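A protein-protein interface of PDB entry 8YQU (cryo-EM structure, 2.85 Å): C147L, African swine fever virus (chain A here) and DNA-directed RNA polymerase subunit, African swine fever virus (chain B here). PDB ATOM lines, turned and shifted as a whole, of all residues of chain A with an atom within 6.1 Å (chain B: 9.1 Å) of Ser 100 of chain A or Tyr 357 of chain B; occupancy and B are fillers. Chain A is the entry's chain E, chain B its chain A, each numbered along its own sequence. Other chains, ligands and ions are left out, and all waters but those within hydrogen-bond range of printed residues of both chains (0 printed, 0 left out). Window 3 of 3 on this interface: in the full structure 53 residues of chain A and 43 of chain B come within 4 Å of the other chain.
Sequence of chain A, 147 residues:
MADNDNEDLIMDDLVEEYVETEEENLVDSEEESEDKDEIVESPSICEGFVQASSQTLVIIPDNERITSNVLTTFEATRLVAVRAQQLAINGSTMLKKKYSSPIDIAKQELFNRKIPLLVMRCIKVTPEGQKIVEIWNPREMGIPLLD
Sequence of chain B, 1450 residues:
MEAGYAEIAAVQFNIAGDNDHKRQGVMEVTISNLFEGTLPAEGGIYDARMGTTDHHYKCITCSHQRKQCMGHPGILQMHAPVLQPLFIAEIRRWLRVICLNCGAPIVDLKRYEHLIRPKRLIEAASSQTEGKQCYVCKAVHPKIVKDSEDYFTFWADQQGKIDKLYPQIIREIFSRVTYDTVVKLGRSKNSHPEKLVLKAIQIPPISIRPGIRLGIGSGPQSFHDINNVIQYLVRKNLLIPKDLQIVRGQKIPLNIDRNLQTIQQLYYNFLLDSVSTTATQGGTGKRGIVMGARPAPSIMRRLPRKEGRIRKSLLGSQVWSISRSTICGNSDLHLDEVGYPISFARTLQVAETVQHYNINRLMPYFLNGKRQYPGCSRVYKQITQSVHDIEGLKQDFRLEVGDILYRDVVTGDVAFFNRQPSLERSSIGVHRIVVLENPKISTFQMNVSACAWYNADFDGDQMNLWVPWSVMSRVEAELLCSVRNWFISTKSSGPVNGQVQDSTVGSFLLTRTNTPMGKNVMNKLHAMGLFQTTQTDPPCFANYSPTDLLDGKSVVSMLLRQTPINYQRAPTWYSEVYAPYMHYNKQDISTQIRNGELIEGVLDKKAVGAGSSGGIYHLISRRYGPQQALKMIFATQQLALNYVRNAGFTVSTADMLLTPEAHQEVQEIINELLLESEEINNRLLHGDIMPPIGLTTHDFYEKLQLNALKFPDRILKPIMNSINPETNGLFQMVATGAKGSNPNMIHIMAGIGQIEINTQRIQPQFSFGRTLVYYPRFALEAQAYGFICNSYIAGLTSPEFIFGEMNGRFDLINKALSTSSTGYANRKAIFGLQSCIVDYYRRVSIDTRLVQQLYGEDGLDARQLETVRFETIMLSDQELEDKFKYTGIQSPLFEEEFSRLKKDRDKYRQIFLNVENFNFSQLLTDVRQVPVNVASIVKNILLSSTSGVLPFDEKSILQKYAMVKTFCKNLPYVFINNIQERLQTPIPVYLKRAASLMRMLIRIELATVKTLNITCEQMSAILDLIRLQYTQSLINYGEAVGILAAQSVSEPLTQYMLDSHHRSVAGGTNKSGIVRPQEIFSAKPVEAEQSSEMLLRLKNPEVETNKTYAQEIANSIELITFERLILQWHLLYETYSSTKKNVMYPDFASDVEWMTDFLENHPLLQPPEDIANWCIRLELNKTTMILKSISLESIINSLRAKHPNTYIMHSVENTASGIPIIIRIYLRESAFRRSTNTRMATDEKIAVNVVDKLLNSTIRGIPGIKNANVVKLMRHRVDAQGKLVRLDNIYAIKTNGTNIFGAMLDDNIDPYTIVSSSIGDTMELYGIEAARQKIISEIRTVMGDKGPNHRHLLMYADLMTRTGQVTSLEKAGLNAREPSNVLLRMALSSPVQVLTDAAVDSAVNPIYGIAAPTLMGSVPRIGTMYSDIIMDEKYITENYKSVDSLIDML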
ATOM      1  N   ALA A  84      -0.648  -3.268  30.281  1.00  0.00           N
ATOM      2  CA  ALA A  84      -1.639  -3.326  29.214  1.00  0.00           C
ATOM      3  C   ALA A  84      -1.439  -4.554  28.338  1.00  0.00           C
ATOM      4  O   ALA A  84      -2.408  -5.225  27.968  1.00  0.00           O
ATOM      5  CB  ALA A  84      -1.578  -2.051  28.374  1.00  0.00           C
ATOM      6  N   LEU A  87      -2.563  -7.597  30.292  1.00  0.00           N
ATOM      7  CA  LEU A  87      -4.021  -7.644  30.300  1.00  0.00           C
ATOM      8  C   LEU A  87      -4.561  -8.120  28.959  1.00  0.00           C
ATOM      9  O   LEU A  87      -5.535  -8.878  28.907  1.00  0.00           O
ATOM     10  CB  LEU A  87      -4.588  -6.269  30.648  1.00  0.00           C
ATOM     11  CG  LEU A  87      -4.502  -5.858  32.116  1.00  0.00           C
ATOM     12  CD1 LEU A  87      -4.697  -4.363  32.250  1.00  0.00           C
ATOM     13  CD2 LEU A  87      -5.531  -6.609  32.938  1.00  0.00           C
ATOM     14  N   ALA A  88      -3.945  -7.678  27.861  1.00  0.00           N
ATOM     15  CA  ALA A  88      -4.308  -8.202  26.551  1.00  0.00           C
ATOM     16  C   ALA A  88      -4.035  -9.694  26.444  1.00  0.00           C
ATOM     17  O   ALA A  88      -4.695 -10.380  25.658  1.00  0.00           O
ATOM     18  CB  ALA A  88      -3.554  -7.450  25.455  1.00  0.00           C
ATOM     19  N   ILE A  89      -3.083 -10.213  27.219  1.00  0.00           N
ATOM     20  CA  ILE A  89      -2.819 -11.648  27.239  1.00  0.00           C
ATOM     21  C   ILE A  89      -3.791 -12.342  28.185  1.00  0.00           C
ATOM     22  O   ILE A  89      -4.525 -13.250  27.778  1.00  0.00           O
ATOM     23  CB  ILE A  89      -1.363 -11.948  27.639  1.00  0.00           C
ATOM     24  CG1 ILE A  89      -0.394 -11.403  26.590  1.00  0.00           C
ATOM     25  CG2 ILE A  89      -1.161 -13.444  27.819  1.00  0.00           C
ATOM     26  CD1 ILE A  89       1.059 -11.480  27.007  1.00  0.00           C
ATOM     27  N   GLY A  91      -6.004 -10.684  31.028  1.00  0.00           N
ATOM     28  CA  GLY A  91      -7.248  -9.991  31.283  1.00  0.00           C
ATOM     29  C   GLY A  91      -7.745 -10.051  32.710  1.00  0.00           C
ATOM     30  O   GLY A  91      -8.769  -9.429  33.017  1.00  0.00           O
ATOM     31  N   LYS A  98     -14.880  -0.473  35.305  1.00  0.00           N
ATOM     32  CA  LYS A  98     -14.867  -1.222  34.056  1.00  0.00           C
ATOM     33  C   LYS A  98     -14.476  -0.308  32.904  1.00  0.00           C
ATOM     34  O   LYS A  98     -15.052   0.773  32.740  1.00  0.00           O
ATOM     35  CB  LYS A  98     -16.233  -1.856  33.789  1.00  0.00           C
ATOM     36  CG  LYS A  98     -16.681  -2.825  34.869  1.00  0.00           C
ATOM     37  CD  LYS A  98     -15.775  -4.042  34.927  1.00  0.00           C
ATOM     38  CE  LYS A  98     -16.314  -5.085  35.890  1.00  0.00           C
ATOM     39  NZ  LYS A  98     -16.228  -4.627  37.305  1.00  0.00           N
ATOM     40  N   TYR A  99     -13.500  -0.746  32.112  1.00  0.00           N
ATOM     41  CA  TYR A  99     -13.065  -0.028  30.924  1.00  0.00           C
ATOM     42  C   TYR A  99     -12.910  -1.013  29.774  1.00  0.00           C
ATOM     43  O   TYR A  99     -12.657  -2.203  29.976  1.00  0.00           O
ATOM     44  CB  TYR A  99     -11.744   0.726  31.153  1.00  0.00           C
ATOM     45  CG  TYR A  99     -11.734   1.598  32.390  1.00  0.00           C
ATOM     46  CD1 TYR A  99     -11.526   1.054  33.650  1.00  0.00           C
ATOM     47  CD2 TYR A  99     -11.945   2.967  32.295  1.00  0.00           C
ATOM     48  CE1 TYR A  99     -11.520   1.849  34.777  1.00  0.00           C
ATOM     49  CE2 TYR A  99     -11.943   3.769  33.418  1.00  0.00           C
ATOM     50  CZ  TYR A  99     -11.732   3.204  34.656  1.00  0.00           C
ATOM     51  OH  TYR A  99     -11.726   3.998  35.778  1.00  0.00           O
ATOM     52  N   SER A 100     -13.064  -0.499  28.554  1.00  0.00           N
ATOM     53  CA  SER A 100     -13.063  -1.320  27.351  1.00  0.00           C
ATOM     54  C   SER A 100     -11.744  -1.249  26.591  1.00  0.00           C
ATOM     55  O   SER A 100     -11.735  -1.398  25.364  1.00  0.00           O
ATOM     56  CB  SER A 100     -14.220  -0.914  26.437  1.00  0.00           C
ATOM     57  OG  SER A 100     -14.041   0.403  25.943  1.00  0.00           O
ATOM     58  N   SER A 101     -10.630  -1.023  27.289  1.00  0.00           N
ATOM     59  CA  SER A 101      -9.332  -0.972  26.640  1.00  0.00           C
ATOM     60  C   SER A 101      -8.257  -1.347  27.648  1.00  0.00           C
ATOM     61  O   SER A 101      -8.321  -0.903  28.803  1.00  0.00           O
ATOM     62  CB  SER A 101      -9.040   0.414  26.060  1.00  0.00           C
ATOM     63  OG  SER A 101      -7.760   0.456  25.455  1.00  0.00           O
ATOM     64  N   PRO A 102      -7.274  -2.160  27.252  1.00  0.00           N
ATOM     65  CA  PRO A 102      -6.185  -2.495  28.183  1.00  0.00           C
ATOM     66  C   PRO A 102      -5.390  -1.288  28.635  1.00  0.00           C
ATOM     67  O   PRO A 102      -4.896  -1.272  29.769  1.00  0.00           O
ATOM     68  CB  PRO A 102      -5.319  -3.473  27.374  1.00  0.00           C
ATOM     69  CG  PRO A 102      -6.186  -3.928  26.239  1.00  0.00           C
ATOM     70  CD  PRO A 102      -7.083  -2.779  25.931  1.00  0.00           C
ATOM     71  N   ASP A 104      -6.458   1.836  29.204  1.00  0.00           N
ATOM     72  CA  ASP A 104      -7.179   2.526  30.269  1.00  0.00           C
ATOM     73  C   ASP A 104      -7.128   1.740  31.572  1.00  0.00           C
ATOM     74  O   ASP A 104      -6.946   2.321  32.649  1.00  0.00           O
ATOM     75  CB  ASP A 104      -8.628   2.773  29.849  1.00  0.00           C
ATOM     76  CG  ASP A 104      -8.773   3.974  28.937  1.00  0.00           C
ATOM     77  OD1 ASP A 104      -7.767   4.680  28.716  1.00  0.00           O
ATOM     78  OD2 ASP A 104      -9.894   4.213  28.442  1.00  0.00           O
ATOM     79  N   ILE A 105      -7.286   0.418  31.496  1.00  0.00           N
ATOM     80  CA  ILE A 105      -7.243  -0.402  32.703  1.00  0.00           C
ATOM     81  C   ILE A 105      -5.864  -0.333  33.345  1.00  0.00           C
ATOM     82  O   ILE A 105      -5.740  -0.222  34.569  1.00  0.00           O
ATOM     83  CB  ILE A 105      -7.650  -1.852  32.387  1.00  0.00           C
ATOM     84  CG1 ILE A 105      -9.066  -1.897  31.815  1.00  0.00           C
ATOM     85  CG2 ILE A 105      -7.578  -2.708  33.640  1.00  0.00           C
ATOM     86  CD1 ILE A 105      -9.492  -3.275  31.364  1.00  0.00           C
ATOM     87  N   GLU B 352      -6.067  -5.028  17.763  1.00  0.00           N
ATOM     88  CA  GLU B 352      -6.800  -5.057  19.021  1.00  0.00           C
ATOM     89  C   GLU B 352      -6.986  -6.509  19.439  1.00  0.00           C
ATOM     90  O   GLU B 352      -7.508  -7.318  18.664  1.00  0.00           O
ATOM     91  CB  GLU B 352      -8.154  -4.363  18.884  1.00  0.00           C
ATOM     92  CG  GLU B 352      -8.076  -2.861  18.682  1.00  0.00           C
ATOM     93  CD  GLU B 352      -7.991  -2.100  19.990  1.00  0.00           C
ATOM     94  OE1 GLU B 352      -8.434  -2.642  21.025  1.00  0.00           O
ATOM     95  OE2 GLU B 352      -7.488  -0.959  19.983  1.00  0.00           O
ATOM     96  N   THR B 353      -6.565  -6.837  20.657  1.00  0.00           N
ATOM     97  CA  THR B 353      -6.700  -8.189  21.179  1.00  0.00           C
ATOM     98  C   THR B 353      -8.061  -8.346  21.846  1.00  0.00           C
ATOM     99  O   THR B 353      -8.461  -7.510  22.661  1.00  0.00           O
ATOM    100  CB  THR B 353      -5.583  -8.506  22.174  1.00  0.00           C
ATOM    101  OG1 THR B 353      -4.312  -8.289  21.551  1.00  0.00           O
ATOM    102  CG2 THR B 353      -5.671  -9.955  22.622  1.00  0.00           C
ATOM    103  N   VAL B 354      -8.764  -9.418  21.496  1.00  0.00           N
ATOM    104  CA  VAL B 354     -10.124  -9.638  21.974  1.00  0.00           C
ATOM    105  C   VAL B 354     -10.077 -10.176  23.398  1.00  0.00           C
ATOM    106  O   VAL B 354      -9.425 -11.190  23.669  1.00  0.00           O
ATOM    107  CB  VAL B 354     -10.884 -10.595  21.048  1.00  0.00           C
ATOM    108  CG1 VAL B 354     -12.230 -10.950  21.644  1.00  0.00           C
ATOM    109  CG2 VAL B 354     -11.051  -9.970  19.678  1.00  0.00           C
ATOM    110  N   GLN B 355     -10.772  -9.501  24.308  1.00  0.00           N
ATOM    111  CA  GLN B 355     -10.914  -9.931  25.691  1.00  0.00           C
ATOM    112  C   GLN B 355     -12.361  -9.737  26.125  1.00  0.00           C
ATOM    113  O   GLN B 355     -13.230  -9.372  25.327  1.00  0.00           O
ATOM    114  CB  GLN B 355      -9.957  -9.170  26.617  1.00  0.00           C
ATOM    115  CG  GLN B 355      -8.490  -9.509  26.421  1.00  0.00           C
ATOM    116  CD  GLN B 355      -8.188 -10.966  26.705  1.00  0.00           C
ATOM    117  OE1 GLN B 355      -7.683 -11.686  25.845  1.00  0.00           O
ATOM    118  NE2 GLN B 355      -8.503 -11.410  27.915  1.00  0.00           N
ATOM    119  N   HIS B 356     -12.620  -9.985  27.410  1.00  0.00           N
ATOM    120  CA  HIS B 356     -13.980  -9.887  27.926  1.00  0.00           C
ATOM    121  C   HIS B 356     -14.449  -8.446  28.077  1.00  0.00           C
ATOM    122  O   HIS B 356     -15.659  -8.210  28.156  1.00  0.00           O
ATOM    123  CB  HIS B 356     -14.085 -10.623  29.265  1.00  0.00           C
ATOM    124  CG  HIS B 356     -13.484  -9.880  30.419  1.00  0.00           C
ATOM    125  ND1 HIS B 356     -12.247 -10.192  30.940  1.00  0.00           N
ATOM    126  CD2 HIS B 356     -13.960  -8.857  31.169  1.00  0.00           C
ATOM    127  CE1 HIS B 356     -11.980  -9.385  31.950  1.00  0.00           C
ATOM    128  NE2 HIS B 356     -13.002  -8.565  32.110  1.00  0.00           N
ATOM    129  N   TYR B 357     -13.532  -7.480  28.121  1.00  0.00           N
ATOM    130  CA  TYR B 357     -13.930  -6.092  28.314  1.00  0.00           C
ATOM    131  C   TYR B 357     -14.199  -5.361  27.006  1.00  0.00           C
ATOM    132  O   TYR B 357     -15.031  -4.447  26.977  1.00  0.00           O
ATOM    133  CB  TYR B 357     -12.864  -5.334  29.113  1.00  0.00           C
ATOM    134  CG  TYR B 357     -11.435  -5.671  28.749  1.00  0.00           C
ATOM    135  CD1 TYR B 357     -10.859  -5.177  27.586  1.00  0.00           C
ATOM    136  CD2 TYR B 357     -10.658  -6.470  29.575  1.00  0.00           C
ATOM    137  CE1 TYR B 357      -9.555  -5.477  27.252  1.00  0.00           C
ATOM    138  CE2 TYR B 357      -9.350  -6.774  29.249  1.00  0.00           C
ATOM    139  CZ  TYR B 357      -8.805  -6.275  28.087  1.00  0.00           C
ATOM    140  OH  TYR B 357      -7.505  -6.575  27.756  1.00  0.00           O
ATOM    141  N   ASN B 358     -13.523  -5.739  25.920  1.00  0.00           N
ATOM    142  CA  ASN B 358     -13.672  -5.066  24.636  1.00  0.00           C
ATOM    143  C   ASN B 358     -14.372  -5.936  23.596  1.00  0.00           C
ATOM    144  O   ASN B 358     -14.299  -5.642  22.399  1.00  0.00           O
ATOM    145  CB  ASN B 358     -12.309  -4.606  24.118  1.00  0.00           C
ATOM    146  CG  ASN B 358     -11.328  -5.749  23.955  1.00  0.00           C
ATOM    147  OD1 ASN B 358     -11.628  -6.896  24.285  1.00  0.00           O
ATOM    148  ND2 ASN B 358     -10.142  -5.439  23.444  1.00  0.00           N
ATOM    149  N   ILE B 359     -15.045  -7.003  24.028  1.00  0.00           N
ATOM    150  CA  ILE B 359     -15.787  -7.840  23.090  1.00  0.00           C
ATOM    151  C   ILE B 359     -16.953  -7.068  22.483  1.00  0.00           C
ATOM    152  O   ILE B 359     -17.266  -7.225  21.297  1.00  0.00           O
ATOM    153  CB  ILE B 359     -16.247  -9.141  23.779  1.00  0.00           C
ATOM    154  CG1 ILE B 359     -16.803 -10.133  22.753  1.00  0.00           C
ATOM    155  CG2 ILE B 359     -17.251  -8.863  24.892  1.00  0.00           C
ATOM    156  CD1 ILE B 359     -15.785 -10.648  21.770  1.00  0.00           C
ATOM    157  N   ASN B 360     -17.612  -6.221  23.277  1.00  0.00           N
ATOM    158  CA  ASN B 360     -18.754  -5.466  22.776  1.00  0.00           C
ATOM    159  C   ASN B 360     -18.334  -4.276  21.923  1.00  0.00           C
ATOM    160  O   ASN B 360     -19.024  -3.942  20.954  1.00  0.00           O
ATOM    161  CB  ASN B 360     -19.625  -4.995  23.941  1.00  0.00           C
ATOM    162  CG  ASN B 360     -20.183  -6.147  24.751  1.00  0.00           C
ATOM    163  OD1 ASN B 360     -20.502  -7.204  24.208  1.00  0.00           O
ATOM    164  ND2 ASN B 360     -20.304  -5.947  26.057  1.00  0.00           N
ATOM    165  N   ARG B 361     -17.221  -3.623  22.264  1.00  0.00           N
ATOM    166  CA  ARG B 361     -16.797  -2.449  21.508  1.00  0.00           C
ATOM    167  C   ARG B 361     -16.220  -2.839  20.153  1.00  0.00           C
ATOM    168  O   ARG B 361     -16.496  -2.183  19.142  1.00  0.00           O
ATOM    169  CB  ARG B 361     -15.772  -1.648  22.309  1.00  0.00           C
ATOM    170  CG  ARG B 361     -15.153  -0.497  21.535  1.00  0.00           C
ATOM    171  CD  ARG B 361     -14.118   0.239  22.365  1.00  0.00           C
ATOM    172  NE  ARG B 361     -13.058  -0.648  22.830  1.00  0.00           N
ATOM    173  CZ  ARG B 361     -12.018  -1.020  22.098  1.00  0.00           C
ATOM    174  NH1 ARG B 361     -11.865  -0.603  20.852  1.00  0.00           N
ATOM    175  NH2 ARG B 361     -11.108  -1.831  22.629  1.00  0.00           N
ATOM    176  N   LEU B 362     -15.412  -3.897  20.112  1.00  0.00           N
ATOM    177  CA  LEU B 362     -14.787  -4.337  18.873  1.00  0.00           C
ATOM    178  C   LEU B 362     -15.751  -5.055  17.941  1.00  0.00           C
ATOM    179  O   LEU B 362     -15.432  -5.227  16.761  1.00  0.00           O
ATOM    180  CB  LEU B 362     -13.605  -5.257  19.179  1.00  0.00           C
ATOM    181  CG  LEU B 362     -12.364  -4.592  19.768  1.00  0.00           C
ATOM    182  CD1 LEU B 362     -11.373  -5.644  20.233  1.00  0.00           C
ATOM    183  CD2 LEU B 362     -11.731  -3.663  18.748  1.00  0.00           C
ATOM    184  N   MET B 363     -16.906  -5.485  18.443  1.00  0.00           N
ATOM    185  CA  MET B 363     -17.823  -6.277  17.625  1.00  0.00           C
ATOM    186  C   MET B 363     -18.369  -5.514  16.422  1.00  0.00           C
ATOM    187  O   MET B 363     -18.432  -6.104  15.329  1.00  0.00           O
ATOM    188  CB  MET B 363     -18.946  -6.826  18.509  1.00  0.00           C
ATOM    189  CG  MET B 363     -19.824  -7.816  17.793  1.00  0.00           C
ATOM    190  SD  MET B 363     -18.898  -9.300  17.376  1.00  0.00           S
ATOM    191  CE  MET B 363     -19.861  -9.887  15.994  1.00  0.00           C
ATOM    192  N   TYR B 365     -16.883  -3.372  14.633  1.00  0.00           N
ATOM    193  CA  TYR B 365     -15.811  -3.408  13.641  1.00  0.00           C
ATOM    194  C   TYR B 365     -15.809  -4.731  12.888  1.00  0.00           C
ATOM    195  O   TYR B 365     -15.594  -4.763  11.671  1.00  0.00           O
ATOM    196  CB  TYR B 365     -14.459  -3.184  14.317  1.00  0.00           C
ATOM    197  CG  TYR B 365     -14.282  -1.817  14.936  1.00  0.00           C
ATOM    198  CD1 TYR B 365     -13.926  -0.723  14.162  1.00  0.00           C
ATOM    199  CD2 TYR B 365     -14.459  -1.625  16.298  1.00  0.00           C
ATOM    200  CE1 TYR B 365     -13.759   0.526  14.725  1.00  0.00           C
ATOM    201  CE2 TYR B 365     -14.294  -0.380  16.871  1.00  0.00           C
ATOM    202  CZ  TYR B 365     -13.944   0.691  16.080  1.00  0.00           C
ATOM    203  OH  TYR B 365     -13.779   1.933  16.647  1.00  0.00           O
ATOM    204  N   ARG B 398     -19.893 -14.224  16.743  1.00  0.00           N
ATOM    205  CA  ARG B 398     -19.025 -13.278  17.435  1.00  0.00           C
ATOM    206  C   ARG B 398     -17.593 -13.792  17.354  1.00  0.00           C
ATOM    207  O   ARG B 398     -17.271 -14.676  16.553  1.00  0.00           O
ATOM    208  CB  ARG B 398     -19.465 -13.062  18.891  1.00  0.00           C
ATOM    209  CG  ARG B 398     -20.925 -12.692  19.077  1.00  0.00           C
ATOM    210  CD  ARG B 398     -21.357 -12.872  20.522  1.00  0.00           C
ATOM    211  NE  ARG B 398     -20.709 -11.904  21.401  1.00  0.00           N
ATOM    212  CZ  ARG B 398     -21.069 -10.633  21.512  1.00  0.00           C
ATOM    213  NH1 ARG B 398     -22.078 -10.136  20.814  1.00  0.00           N
ATOM    214  NH2 ARG B 398     -20.401  -9.840  22.344  1.00  0.00           N
ATOM    215  N   VAL B 401     -12.484 -15.273  22.593  1.00  0.00           N
ATOM    216  CA  VAL B 401     -11.616 -14.514  23.484  1.00  0.00           C
ATOM    217  C   VAL B 401     -10.168 -14.905  23.234  1.00  0.00           C
ATOM    218  O   VAL B 401      -9.825 -16.093  23.180  1.00  0.00           O
ATOM    219  CB  VAL B 401     -12.022 -14.744  24.946  1.00  0.00           C
ATOM    220  CG1 VAL B 401     -10.941 -14.245  25.890  1.00  0.00           C
ATOM    221  CG2 VAL B 401     -13.347 -14.056  25.239  1.00  0.00           C
ATOM    222  N   GLY B 402      -9.308 -13.901  23.080  1.00  0.00           N
ATOM    223  CA  GLY B 402      -7.911 -14.107  22.756  1.00  0.00           C
ATOM    224  C   GLY B 402      -7.553 -13.805  21.319  1.00  0.00           C
ATOM    225  O   GLY B 402      -6.361 -13.717  21.003  1.00  0.00           O
ATOM    226  N   ARG B 407      -8.470  -3.818  13.004  1.00  0.00           N
ATOM    227  CA  ARG B 407      -9.548  -2.926  12.618  1.00  0.00           C
ATOM    228  C   ARG B 407      -9.007  -1.702  11.884  1.00  0.00           C
ATOM    229  O   ARG B 407      -7.809  -1.415  11.891  1.00  0.00           O
ATOM    230  CB  ARG B 407     -10.346  -2.495  13.847  1.00  0.00           C
ATOM    231  CG  ARG B 407      -9.540  -1.691  14.850  1.00  0.00           C
ATOM    232  CD  ARG B 407     -10.439  -1.020  15.868  1.00  0.00           C
ATOM    233  NE  ARG B 407      -9.682  -0.226  16.828  1.00  0.00           N
ATOM    234  CZ  ARG B 407      -9.199   0.984  16.582  1.00  0.00           C
ATOM    235  NH1 ARG B 407      -9.368   1.571  15.408  1.00  0.00           N
ATOM    236  NH2 ARG B 407      -8.532   1.623  17.538  1.00  0.00           N
ATOM    237  N   VAL B 471       0.051  -2.820  21.388  1.00  0.00           N
ATOM    238  CA  VAL B 471      -0.410  -2.173  22.613  1.00  0.00           C
ATOM    239  C   VAL B 471       0.741  -1.449  23.299  1.00  0.00           C
ATOM    240  O   VAL B 471       0.578  -0.333  23.805  1.00  0.00           O
ATOM    241  CB  VAL B 471      -1.068  -3.203  23.549  1.00  0.00           C
ATOM    242  CG1 VAL B 471      -1.729  -2.501  24.720  1.00  0.00           C
ATOM    243  CG2 VAL B 471      -2.080  -4.038  22.786  1.00  0.00           C
ATOM    244  N   ARG B 474       1.473   1.647  21.379  1.00  0.00           N
ATOM    245  CA  ARG B 474       0.345   2.570  21.441  1.00  0.00           C
ATOM    246  C   ARG B 474       0.268   3.265  22.794  1.00  0.00           C
ATOM    247  O   ARG B 474      -0.147   4.427  22.873  1.00  0.00           O
ATOM    248  CB  ARG B 474      -0.953   1.822  21.144  1.00  0.00           C
ATOM    249  CG  ARG B 474      -2.091   2.702  20.672  1.00  0.00           C
ATOM    250  CD  ARG B 474      -3.095   1.901  19.861  1.00  0.00           C
ATOM    251  NE  ARG B 474      -3.801   0.920  20.674  1.00  0.00           N
ATOM    252  CZ  ARG B 474      -3.788  -0.387  20.448  1.00  0.00           C
ATOM    253  NH1 ARG B 474      -3.109  -0.906  19.439  1.00  0.00           N
ATOM    254  NH2 ARG B 474      -4.477  -1.191  21.253  1.00  0.00           N
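The side-chain hydroxyl (OH) of Tyr 357 of chain B sits at hydrogen-bond distance from the backbone carbonyl oxygen (O) of Leu 87 of chain A (3.2 Å).
The guanidinium group (NH2) of Arg 361 of chain B is in hydrogen-bond range of the backbone carbonyl oxygen (O) of Ser 100 of chain A (2.8 Å).
The side-chain amide oxygen (OE1) of Gln 355 of chain B lies close to the backbone carbonyl oxygen (O) of Ala 88 of chain A.
The side-chain carboxylate (OE1) of Glu 352 of chain B is in salt-bridge range of the guanidinium group (NH2) of Arg 361 of chain B (3.2 Å).
The side-chain amide oxygen (OD1) of Asn 358 of chain B is in hydrogen-bond range of the backbone NH (N) of Gln 355 of chain B, at 2.7 Å.
O of Thr 353 of chain B is in hydrogen-bond range of ND2 of Asn 358 of chain B (2.8 Å).
Among the printed residues, merely in contact across the chains: Ala 84 of chain A with Val 471 of chain B (3.7 Å), Leu 87 of chain A with Gln 355 of chain B (3.9 Å), Ala 88 of chain A with Thr 353 of chain B (3.2 Å), Ala 88 of chain A with Tyr 357 of chain B (3.7 Å), Gly 91 of chain A with Gln 355 of chain B (3.9 Å), Gly 91 of chain A with His 356 of chain B (3.4 Å), Tyr 99 of chain A with Tyr 357 of chain B (3.3 Å), Ser 100 of chain A with Tyr 357 of chain B (3.7 Å), Ser 100 of chain A with Asn 358 of chain B (3.5 Å), Pro 102 of chain A with Tyr 357 of chain B (3.3 Å) and Ile 105 of chain A with Tyr 357 of chain B (3.8 Å).
Printed residues of chain B within 4 Å of Leu 87 of chain A: Gln 355 (3.9 Å) and Tyr 357 (3.2 Å).
Of the printed residues of chain B, Gly 91 of chain A touches Gln 355 and His 356.
Ser 100 of chain A touches just these residues of chain B: Tyr 357 (3.7 Å), Asn 358 (3.5 Å) and Arg 361 (2.8 Å).
No residue of chain B comes within 4 Å of Ser 101 of chain A.
Printed residues of chain B within 4 Å of Ile 105 of chain A: Tyr 357 (3.8 Å).
Of the printed residues of chain A, Gln 355 of chain B touches Leu 87 (3.9 Å), Ala 88 (3.3 Å) and Gly 91 (3.9 Å).
Of chain A, only Leu 87, Ala 88, Tyr 99, Ser 100, Pro 102 and Ile 105 come within 4 Å of Tyr 357 of chain B.
Of the printed residues of chain A, Val 471 of chain B touches Ala 84 (3.7 Å).
The nearest residue of chain A that does not touch Tyr 357 of chain B is Ser 101 of chain A (4.2 Å).
The nearest printed residue of chain A that does not touch Val 471 of chain B is Pro 102 of chain A (4.6 Å).
Hydrophobic or aromatic side chains of chain B within 4 Å of the printed part of chain A: His 356, Tyr 357 and Val 471.
Of the 12 printed residues of chain A, 8 touch a printed residue of chain B.
Hydrophobic or aromatic side chains of chain A within 4 Å of the printed part of chain B: Ala 84, Ala 88, Pro 102 and Ile 105.
Among the printed residues, no Asp or Glu carboxylate lies within 4 Å of a Lys or Arg side-chain nitrogen of the other chain.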
